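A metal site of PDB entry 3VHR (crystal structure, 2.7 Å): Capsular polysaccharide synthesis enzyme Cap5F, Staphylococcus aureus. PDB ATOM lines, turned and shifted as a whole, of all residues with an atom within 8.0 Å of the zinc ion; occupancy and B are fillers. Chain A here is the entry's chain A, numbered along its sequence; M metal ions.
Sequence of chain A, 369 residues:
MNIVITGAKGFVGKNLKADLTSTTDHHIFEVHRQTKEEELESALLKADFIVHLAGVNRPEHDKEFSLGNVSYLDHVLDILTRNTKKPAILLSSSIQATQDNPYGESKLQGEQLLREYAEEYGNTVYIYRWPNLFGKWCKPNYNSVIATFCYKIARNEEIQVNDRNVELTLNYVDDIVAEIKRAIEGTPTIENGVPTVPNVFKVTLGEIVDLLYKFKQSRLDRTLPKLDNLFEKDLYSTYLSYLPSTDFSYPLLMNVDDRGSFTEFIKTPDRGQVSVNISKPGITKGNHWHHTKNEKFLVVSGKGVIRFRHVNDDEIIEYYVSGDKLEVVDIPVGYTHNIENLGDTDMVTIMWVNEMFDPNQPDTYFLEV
The backbone carbonyl oxygen (O) of Tyr 335 lies within hydrogen-bond range of a ring nitrogen (ND1) of His 337, 2.8 Å away. O of His 337 sits at hydrogen-bond distance from N of Asn 287 (2.8 Å). N of His 337 sits at hydrogen-bond distance from O of His 288 (3.0 Å). The backbone carbonyl oxygen (O) of His 288 sits close to the side-chain hydroxyl (OG1) of Thr 336 (3.2 Å). O of Asp 363 is in hydrogen-bond range of ND1 of His 290 (2.7 Å). The backbone carbonyl oxygen (O) of Glu 295 lies within hydrogen-bond range of the backbone NH (N) of Ile 331, 2.9 Å away.
NE2 of His 288 touches the zinc ion, 2.9 Å away. Within 4 Å of the zinc ion: His 288, His 290, Glu 295 and His 337. The nearest printed residue that does not touch the zinc ion is Ile 331 (4.6 Å).
The zinc ion is bound by NE2 of His 337 (2.1 Å), NE2 of His 290 (2.1 Å) and OE1 of Glu 295 (2.2 Å). Slightly farther from the zinc ion lies OE2 of Glu 295 (2.8 Å).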
ATOM      1  N   GLY A 286      -0.049  25.066  -0.815  1.00  0.00           N
ATOM      2  CA  GLY A 286      -1.134  25.071   0.144  1.00  0.00           C
ATOM      3  C   GLY A 286      -0.638  24.744   1.528  1.00  0.00           C
ATOM      4  O   GLY A 286       0.196  25.461   2.068  1.00  0.00           O
ATOM      5  N   ASN A 287      -1.150  23.634   2.081  1.00  0.00           N
ATOM      6  CA  ASN A 287      -0.885  23.261   3.472  1.00  0.00           C
ATOM      7  C   ASN A 287      -1.321  24.342   4.451  1.00  0.00           C
ATOM      8  O   ASN A 287      -0.601  24.647   5.403  1.00  0.00           O
ATOM      9  CB  ASN A 287       0.584  22.904   3.691  1.00  0.00           C
ATOM     10  CG  ASN A 287       0.967  21.580   3.077  1.00  0.00           C
ATOM     11  OD1 ASN A 287       0.288  20.555   3.262  1.00  0.00           O
ATOM     12  ND2 ASN A 287       2.074  21.559   2.356  1.00  0.00           N
ATOM     13  N   HIS A 288      -2.479  24.938   4.218  1.00  0.00           N
ATOM     14  CA  HIS A 288      -3.050  25.894   5.164  1.00  0.00           C
ATOM     15  C   HIS A 288      -4.513  25.660   5.440  1.00  0.00           C
ATOM     16  O   HIS A 288      -5.174  24.870   4.762  1.00  0.00           O
ATOM     17  CB  HIS A 288      -2.777  27.343   4.715  1.00  0.00           C
ATOM     18  CG  HIS A 288      -3.172  27.644   3.271  1.00  0.00           C
ATOM     19  ND1 HIS A 288      -2.325  28.239   2.403  1.00  0.00           N
ATOM     20  CD2 HIS A 288      -4.372  27.451   2.573  1.00  0.00           C
ATOM     21  CE1 HIS A 288      -2.938  28.412   1.212  1.00  0.00           C
ATOM     22  NE2 HIS A 288      -4.194  27.933   1.321  1.00  0.00           N
ATOM     23  N   TRP A 289      -5.049  26.296   6.464  1.00  0.00           N
ATOM     24  CA  TRP A 289      -6.490  26.256   6.672  1.00  0.00           C
ATOM     25  C   TRP A 289      -7.034  27.640   6.889  1.00  0.00           C
ATOM     26  O   TRP A 289      -6.269  28.584   7.151  1.00  0.00           O
ATOM     27  CB  TRP A 289      -6.876  25.280   7.781  1.00  0.00           C
ATOM     28  CG  TRP A 289      -6.340  25.635   9.136  1.00  0.00           C
ATOM     29  CD1 TRP A 289      -5.070  25.397   9.640  1.00  0.00           C
ATOM     30  CD2 TRP A 289      -7.054  26.314  10.218  1.00  0.00           C
ATOM     31  NE1 TRP A 289      -4.960  25.864  10.922  1.00  0.00           N
ATOM     32  CE2 TRP A 289      -6.112  26.437  11.324  1.00  0.00           C
ATOM     33  CE3 TRP A 289      -8.346  26.831  10.368  1.00  0.00           C
ATOM     34  CZ2 TRP A 289      -6.454  27.043  12.525  1.00  0.00           C
ATOM     35  CZ3 TRP A 289      -8.676  27.431  11.574  1.00  0.00           C
ATOM     36  CH2 TRP A 289      -7.756  27.531  12.631  1.00  0.00           C
ATOM     37  N   HIS A 290      -8.348  27.784   6.764  1.00  0.00           N
ATOM     38  CA  HIS A 290      -8.995  29.072   6.911  1.00  0.00           C
ATOM     39  C   HIS A 290     -10.095  28.989   7.924  1.00  0.00           C
ATOM     40  O   HIS A 290     -10.676  27.915   8.096  1.00  0.00           O
ATOM     41  CB  HIS A 290      -9.603  29.506   5.578  1.00  0.00           C
ATOM     42  CG  HIS A 290      -8.651  29.439   4.409  1.00  0.00           C
ATOM     43  ND1 HIS A 290      -7.574  30.236   4.299  1.00  0.00           N
ATOM     44  CD2 HIS A 290      -8.681  28.661   3.263  1.00  0.00           C
ATOM     45  CE1 HIS A 290      -6.930  29.957   3.157  1.00  0.00           C
ATOM     46  NE2 HIS A 290      -7.611  29.001   2.515  1.00  0.00           N
ATOM     47  N   LYS A 293     -12.653  32.029   5.092  1.00  0.00           N
ATOM     48  CA  LYS A 293     -12.329  31.995   3.674  1.00  0.00           C
ATOM     49  C   LYS A 293     -12.594  30.592   3.139  1.00  0.00           C
ATOM     50  O   LYS A 293     -12.219  29.595   3.773  1.00  0.00           O
ATOM     51  CB  LYS A 293     -10.857  32.354   3.466  1.00  0.00           C
ATOM     52  CG  LYS A 293     -10.489  32.741   2.042  1.00  0.00           C
ATOM     53  CD  LYS A 293      -8.981  32.813   1.848  1.00  0.00           C
ATOM     54  CE  LYS A 293      -8.367  34.012   2.556  1.00  0.00           C
ATOM     55  NZ  LYS A 293      -8.719  35.255   1.826  1.00  0.00           N
ATOM     56  N   ASN A 294     -13.258  30.487   1.999  1.00  0.00           N
ATOM     57  CA  ASN A 294     -13.355  29.194   1.340  1.00  0.00           C
ATOM     58  C   ASN A 294     -13.203  29.312  -0.160  1.00  0.00           C
ATOM     59  O   ASN A 294     -13.311  30.410  -0.732  1.00  0.00           O
ATOM     60  CB  ASN A 294     -14.632  28.462   1.716  1.00  0.00           C
ATOM     61  CG  ASN A 294     -15.865  29.118   1.175  1.00  0.00           C
ATOM     62  OD1 ASN A 294     -16.588  29.787   1.916  1.00  0.00           O
ATOM     63  ND2 ASN A 294     -16.139  28.920  -0.109  1.00  0.00           N
ATOM     64  N   GLU A 295     -12.924  28.181  -0.809  1.00  0.00           N
ATOM     65  CA  GLU A 295     -12.559  28.211  -2.207  1.00  0.00           C
ATOM     66  C   GLU A 295     -13.275  27.155  -3.037  1.00  0.00           C
ATOM     67  O   GLU A 295     -13.959  26.265  -2.500  1.00  0.00           O
ATOM     68  CB  GLU A 295     -11.046  28.108  -2.334  1.00  0.00           C
ATOM     69  CG  GLU A 295     -10.335  29.212  -1.576  1.00  0.00           C
ATOM     70  CD  GLU A 295      -9.046  28.763  -0.914  1.00  0.00           C
ATOM     71  OE1 GLU A 295      -9.035  27.781  -0.126  1.00  0.00           O
ATOM     72  OE2 GLU A 295      -8.030  29.423  -1.179  1.00  0.00           O
ATOM     73  N   PHE A 297     -11.912  24.848  -6.325  1.00  0.00           N
ATOM     74  CA  PHE A 297     -10.807  24.527  -7.231  1.00  0.00           C
ATOM     75  C   PHE A 297     -11.287  23.806  -8.480  1.00  0.00           C
ATOM     76  O   PHE A 297     -11.982  22.789  -8.400  1.00  0.00           O
ATOM     77  CB  PHE A 297      -9.731  23.698  -6.535  1.00  0.00           C
ATOM     78  CG  PHE A 297      -9.010  24.432  -5.438  1.00  0.00           C
ATOM     79  CD1 PHE A 297      -9.202  25.809  -5.242  1.00  0.00           C
ATOM     80  CD2 PHE A 297      -8.106  23.763  -4.606  1.00  0.00           C
ATOM     81  CE1 PHE A 297      -8.519  26.482  -4.236  1.00  0.00           C
ATOM     82  CE2 PHE A 297      -7.427  24.424  -3.610  1.00  0.00           C
ATOM     83  CZ  PHE A 297      -7.635  25.786  -3.418  1.00  0.00           C
ATOM     84  N   ILE A 331     -13.499  23.886  -0.962  1.00  0.00           N
ATOM     85  CA  ILE A 331     -12.513  23.802   0.105  1.00  0.00           C
ATOM     86  C   ILE A 331     -13.181  24.300   1.391  1.00  0.00           C
ATOM     87  O   ILE A 331     -13.191  25.500   1.649  1.00  0.00           O
ATOM     88  CB  ILE A 331     -11.273  24.651  -0.213  1.00  0.00           C
ATOM     89  CG1 ILE A 331     -10.767  24.418  -1.652  1.00  0.00           C
ATOM     90  CG2 ILE A 331     -10.210  24.437   0.854  1.00  0.00           C
ATOM     91  CD1 ILE A 331     -10.520  22.967  -2.025  1.00  0.00           C
ATOM     92  N   PRO A 332     -13.751  23.385   2.183  1.00  0.00           N
ATOM     93  CA  PRO A 332     -14.554  23.826   3.318  1.00  0.00           C
ATOM     94  C   PRO A 332     -13.677  24.439   4.383  1.00  0.00           C
ATOM     95  O   PRO A 332     -12.482  24.124   4.448  1.00  0.00           O
ATOM     96  CB  PRO A 332     -15.175  22.521   3.837  1.00  0.00           C
ATOM     97  CG  PRO A 332     -14.918  21.506   2.768  1.00  0.00           C
ATOM     98  CD  PRO A 332     -13.620  21.924   2.170  1.00  0.00           C
ATOM     99  N   TYR A 335     -10.553  22.795   7.355  1.00  0.00           N
ATOM    100  CA  TYR A 335      -9.726  21.703   6.826  1.00  0.00           C
ATOM    101  C   TYR A 335      -8.478  22.274   6.239  1.00  0.00           C
ATOM    102  O   TYR A 335      -8.531  23.128   5.332  1.00  0.00           O
ATOM    103  CB  TYR A 335     -10.427  20.906   5.733  1.00  0.00           C
ATOM    104  CG  TYR A 335     -11.543  20.038   6.222  1.00  0.00           C
ATOM    105  CD1 TYR A 335     -12.799  20.588   6.494  1.00  0.00           C
ATOM    106  CD2 TYR A 335     -11.357  18.682   6.421  1.00  0.00           C
ATOM    107  CE1 TYR A 335     -13.839  19.795   6.951  1.00  0.00           C
ATOM    108  CE2 TYR A 335     -12.391  17.874   6.884  1.00  0.00           C
ATOM    109  CZ  TYR A 335     -13.635  18.449   7.142  1.00  0.00           C
ATOM    110  OH  TYR A 335     -14.675  17.679   7.590  1.00  0.00           O
ATOM    111  N   THR A 336      -7.336  21.821   6.729  1.00  0.00           N
ATOM    112  CA  THR A 336      -6.095  22.160   6.060  1.00  0.00           C
ATOM    113  C   THR A 336      -6.061  21.457   4.705  1.00  0.00           C
ATOM    114  O   THR A 336      -6.577  20.330   4.571  1.00  0.00           O
ATOM    115  CB  THR A 336      -4.849  21.857   6.913  1.00  0.00           C
ATOM    116  OG1 THR A 336      -3.729  22.487   6.300  1.00  0.00           O
ATOM    117  CG2 THR A 336      -4.587  20.348   7.028  1.00  0.00           C
ATOM    118  N   HIS A 337      -5.510  22.126   3.697  1.00  0.00           N
ATOM    119  CA  HIS A 337      -5.577  21.619   2.330  1.00  0.00           C
ATOM    120  C   HIS A 337      -4.371  21.902   1.502  1.00  0.00           C
ATOM    121  O   HIS A 337      -3.789  22.983   1.594  1.00  0.00           O
ATOM    122  CB  HIS A 337      -6.814  22.148   1.638  1.00  0.00           C
ATOM    123  CG  HIS A 337      -7.011  23.631   1.793  1.00  0.00           C
ATOM    124  ND1 HIS A 337      -7.542  24.174   2.907  1.00  0.00           N
ATOM    125  CD2 HIS A 337      -6.731  24.688   0.936  1.00  0.00           C
ATOM    126  CE1 HIS A 337      -7.606  25.507   2.764  1.00  0.00           C
ATOM    127  NE2 HIS A 337      -7.104  25.818   1.556  1.00  0.00           N
ATOM    128  N   ASN A 338      -3.955  20.939   0.674  1.00  0.00           N
ATOM    129  CA  ASN A 338      -2.865  21.170  -0.282  1.00  0.00           C
ATOM    130  C   ASN A 338      -3.160  20.653  -1.686  1.00  0.00           C
ATOM    131  O   ASN A 338      -4.081  19.852  -1.880  1.00  0.00           O
ATOM    132  CB  ASN A 338      -1.492  20.709   0.230  1.00  0.00           C
ATOM    133  CG  ASN A 338      -1.327  19.194   0.295  1.00  0.00           C
ATOM    134  OD1 ASN A 338      -1.838  18.446  -0.529  1.00  0.00           O
ATOM    135  ND2 ASN A 338      -0.596  18.736   1.305  1.00  0.00           N
ATOM    136  N   MET A 351      -9.113  29.130  -9.460  1.00  0.00           N
ATOM    137  CA  MET A 351      -9.434  29.190  -8.028  1.00  0.00           C
ATOM    138  C   MET A 351     -10.413  30.270  -7.761  1.00  0.00           C
ATOM    139  O   MET A 351     -10.137  31.448  -7.993  1.00  0.00           O
ATOM    140  CB  MET A 351      -8.167  29.367  -7.207  1.00  0.00           C
ATOM    141  CG  MET A 351      -7.274  28.145  -7.388  1.00  0.00           C
ATOM    142  SD  MET A 351      -5.710  28.297  -6.194  1.00  0.00           S
ATOM    143  CE  MET A 351      -5.237  26.399  -5.932  1.00  0.00           C
ATOM    144  N   TRP A 352     -11.590  29.891  -7.304  1.00  0.00           N
ATOM    145  CA  TRP A 352     -12.575  30.862  -6.852  1.00  0.00           C
ATOM    146  C   TRP A 352     -12.441  30.988  -5.362  1.00  0.00           C
ATOM    147  O   TRP A 352     -12.247  29.985  -4.677  1.00  0.00           O
ATOM    148  CB  TRP A 352     -13.994  30.450  -7.264  1.00  0.00           C
ATOM    149  CG  TRP A 352     -15.022  31.406  -6.744  1.00  0.00           C
ATOM    150  CD1 TRP A 352     -15.417  32.612  -7.307  1.00  0.00           C
ATOM    151  CD2 TRP A 352     -15.763  31.307  -5.482  1.00  0.00           C
ATOM    152  NE1 TRP A 352     -16.342  33.229  -6.507  1.00  0.00           N
ATOM    153  CE2 TRP A 352     -16.590  32.507  -5.397  1.00  0.00           C
ATOM    154  CE3 TRP A 352     -15.811  30.373  -4.438  1.00  0.00           C
ATOM    155  CZ2 TRP A 352     -17.444  32.740  -4.329  1.00  0.00           C
ATOM    156  CZ3 TRP A 352     -16.672  30.626  -3.364  1.00  0.00           C
ATOM    157  CH2 TRP A 352     -17.470  31.783  -3.312  1.00  0.00           C
ATOM    158  N   VAL A 353     -12.498  32.205  -4.836  1.00  0.00           N
ATOM    159  CA  VAL A 353     -12.432  32.420  -3.390  1.00  0.00           C
ATOM    160  C   VAL A 353     -13.534  33.375  -2.979  1.00  0.00           C
ATOM    161  O   VAL A 353     -13.872  34.286  -3.735  1.00  0.00           O
ATOM    162  CB  VAL A 353     -11.016  32.897  -2.933  1.00  0.00           C
ATOM    163  CG1 VAL A 353     -10.619  34.183  -3.608  1.00  0.00           C
ATOM    164  CG2 VAL A 353     -10.981  33.076  -1.418  1.00  0.00           C
ATOM    165  N   ASP A 363      -6.484  35.400   7.099  1.00  0.00           N
ATOM    166  CA  ASP A 363      -7.264  34.226   7.493  1.00  0.00           C
ATOM    167  C   ASP A 363      -6.722  32.940   6.842  1.00  0.00           C
ATOM    168  O   ASP A 363      -7.449  32.141   6.234  1.00  0.00           O
ATOM    169  CB  ASP A 363      -8.750  34.431   7.182  1.00  0.00           C
ATOM    170  CG  ASP A 363      -9.612  33.356   7.771  1.00  0.00           C
ATOM    171  OD1 ASP A 363      -9.231  32.841   8.850  1.00  0.00           O
ATOM    172  OD2 ASP A 363     -10.639  33.006   7.141  1.00  0.00           O
ATOM    173  N   THR A 364      -5.423  32.745   6.969  1.00  0.00           N
ATOM    174  CA  THR A 364      -4.777  31.564   6.423  1.00  0.00           C
ATOM    175  C   THR A 364      -3.605  31.181   7.341  1.00  0.00           C
ATOM    176  O   THR A 364      -2.732  31.992   7.630  1.00  0.00           O
ATOM    177  CB  THR A 364      -4.449  31.727   4.901  1.00  0.00           C
ATOM    178  OG1 THR A 364      -3.384  30.835   4.530  1.00  0.00           O
ATOM    179  CG2 THR A 364      -4.052  33.103   4.559  1.00  0.00           C
HETATM  180 ZN    ZN M   1      -7.080  27.780   0.893  1.00  0.00          ZN
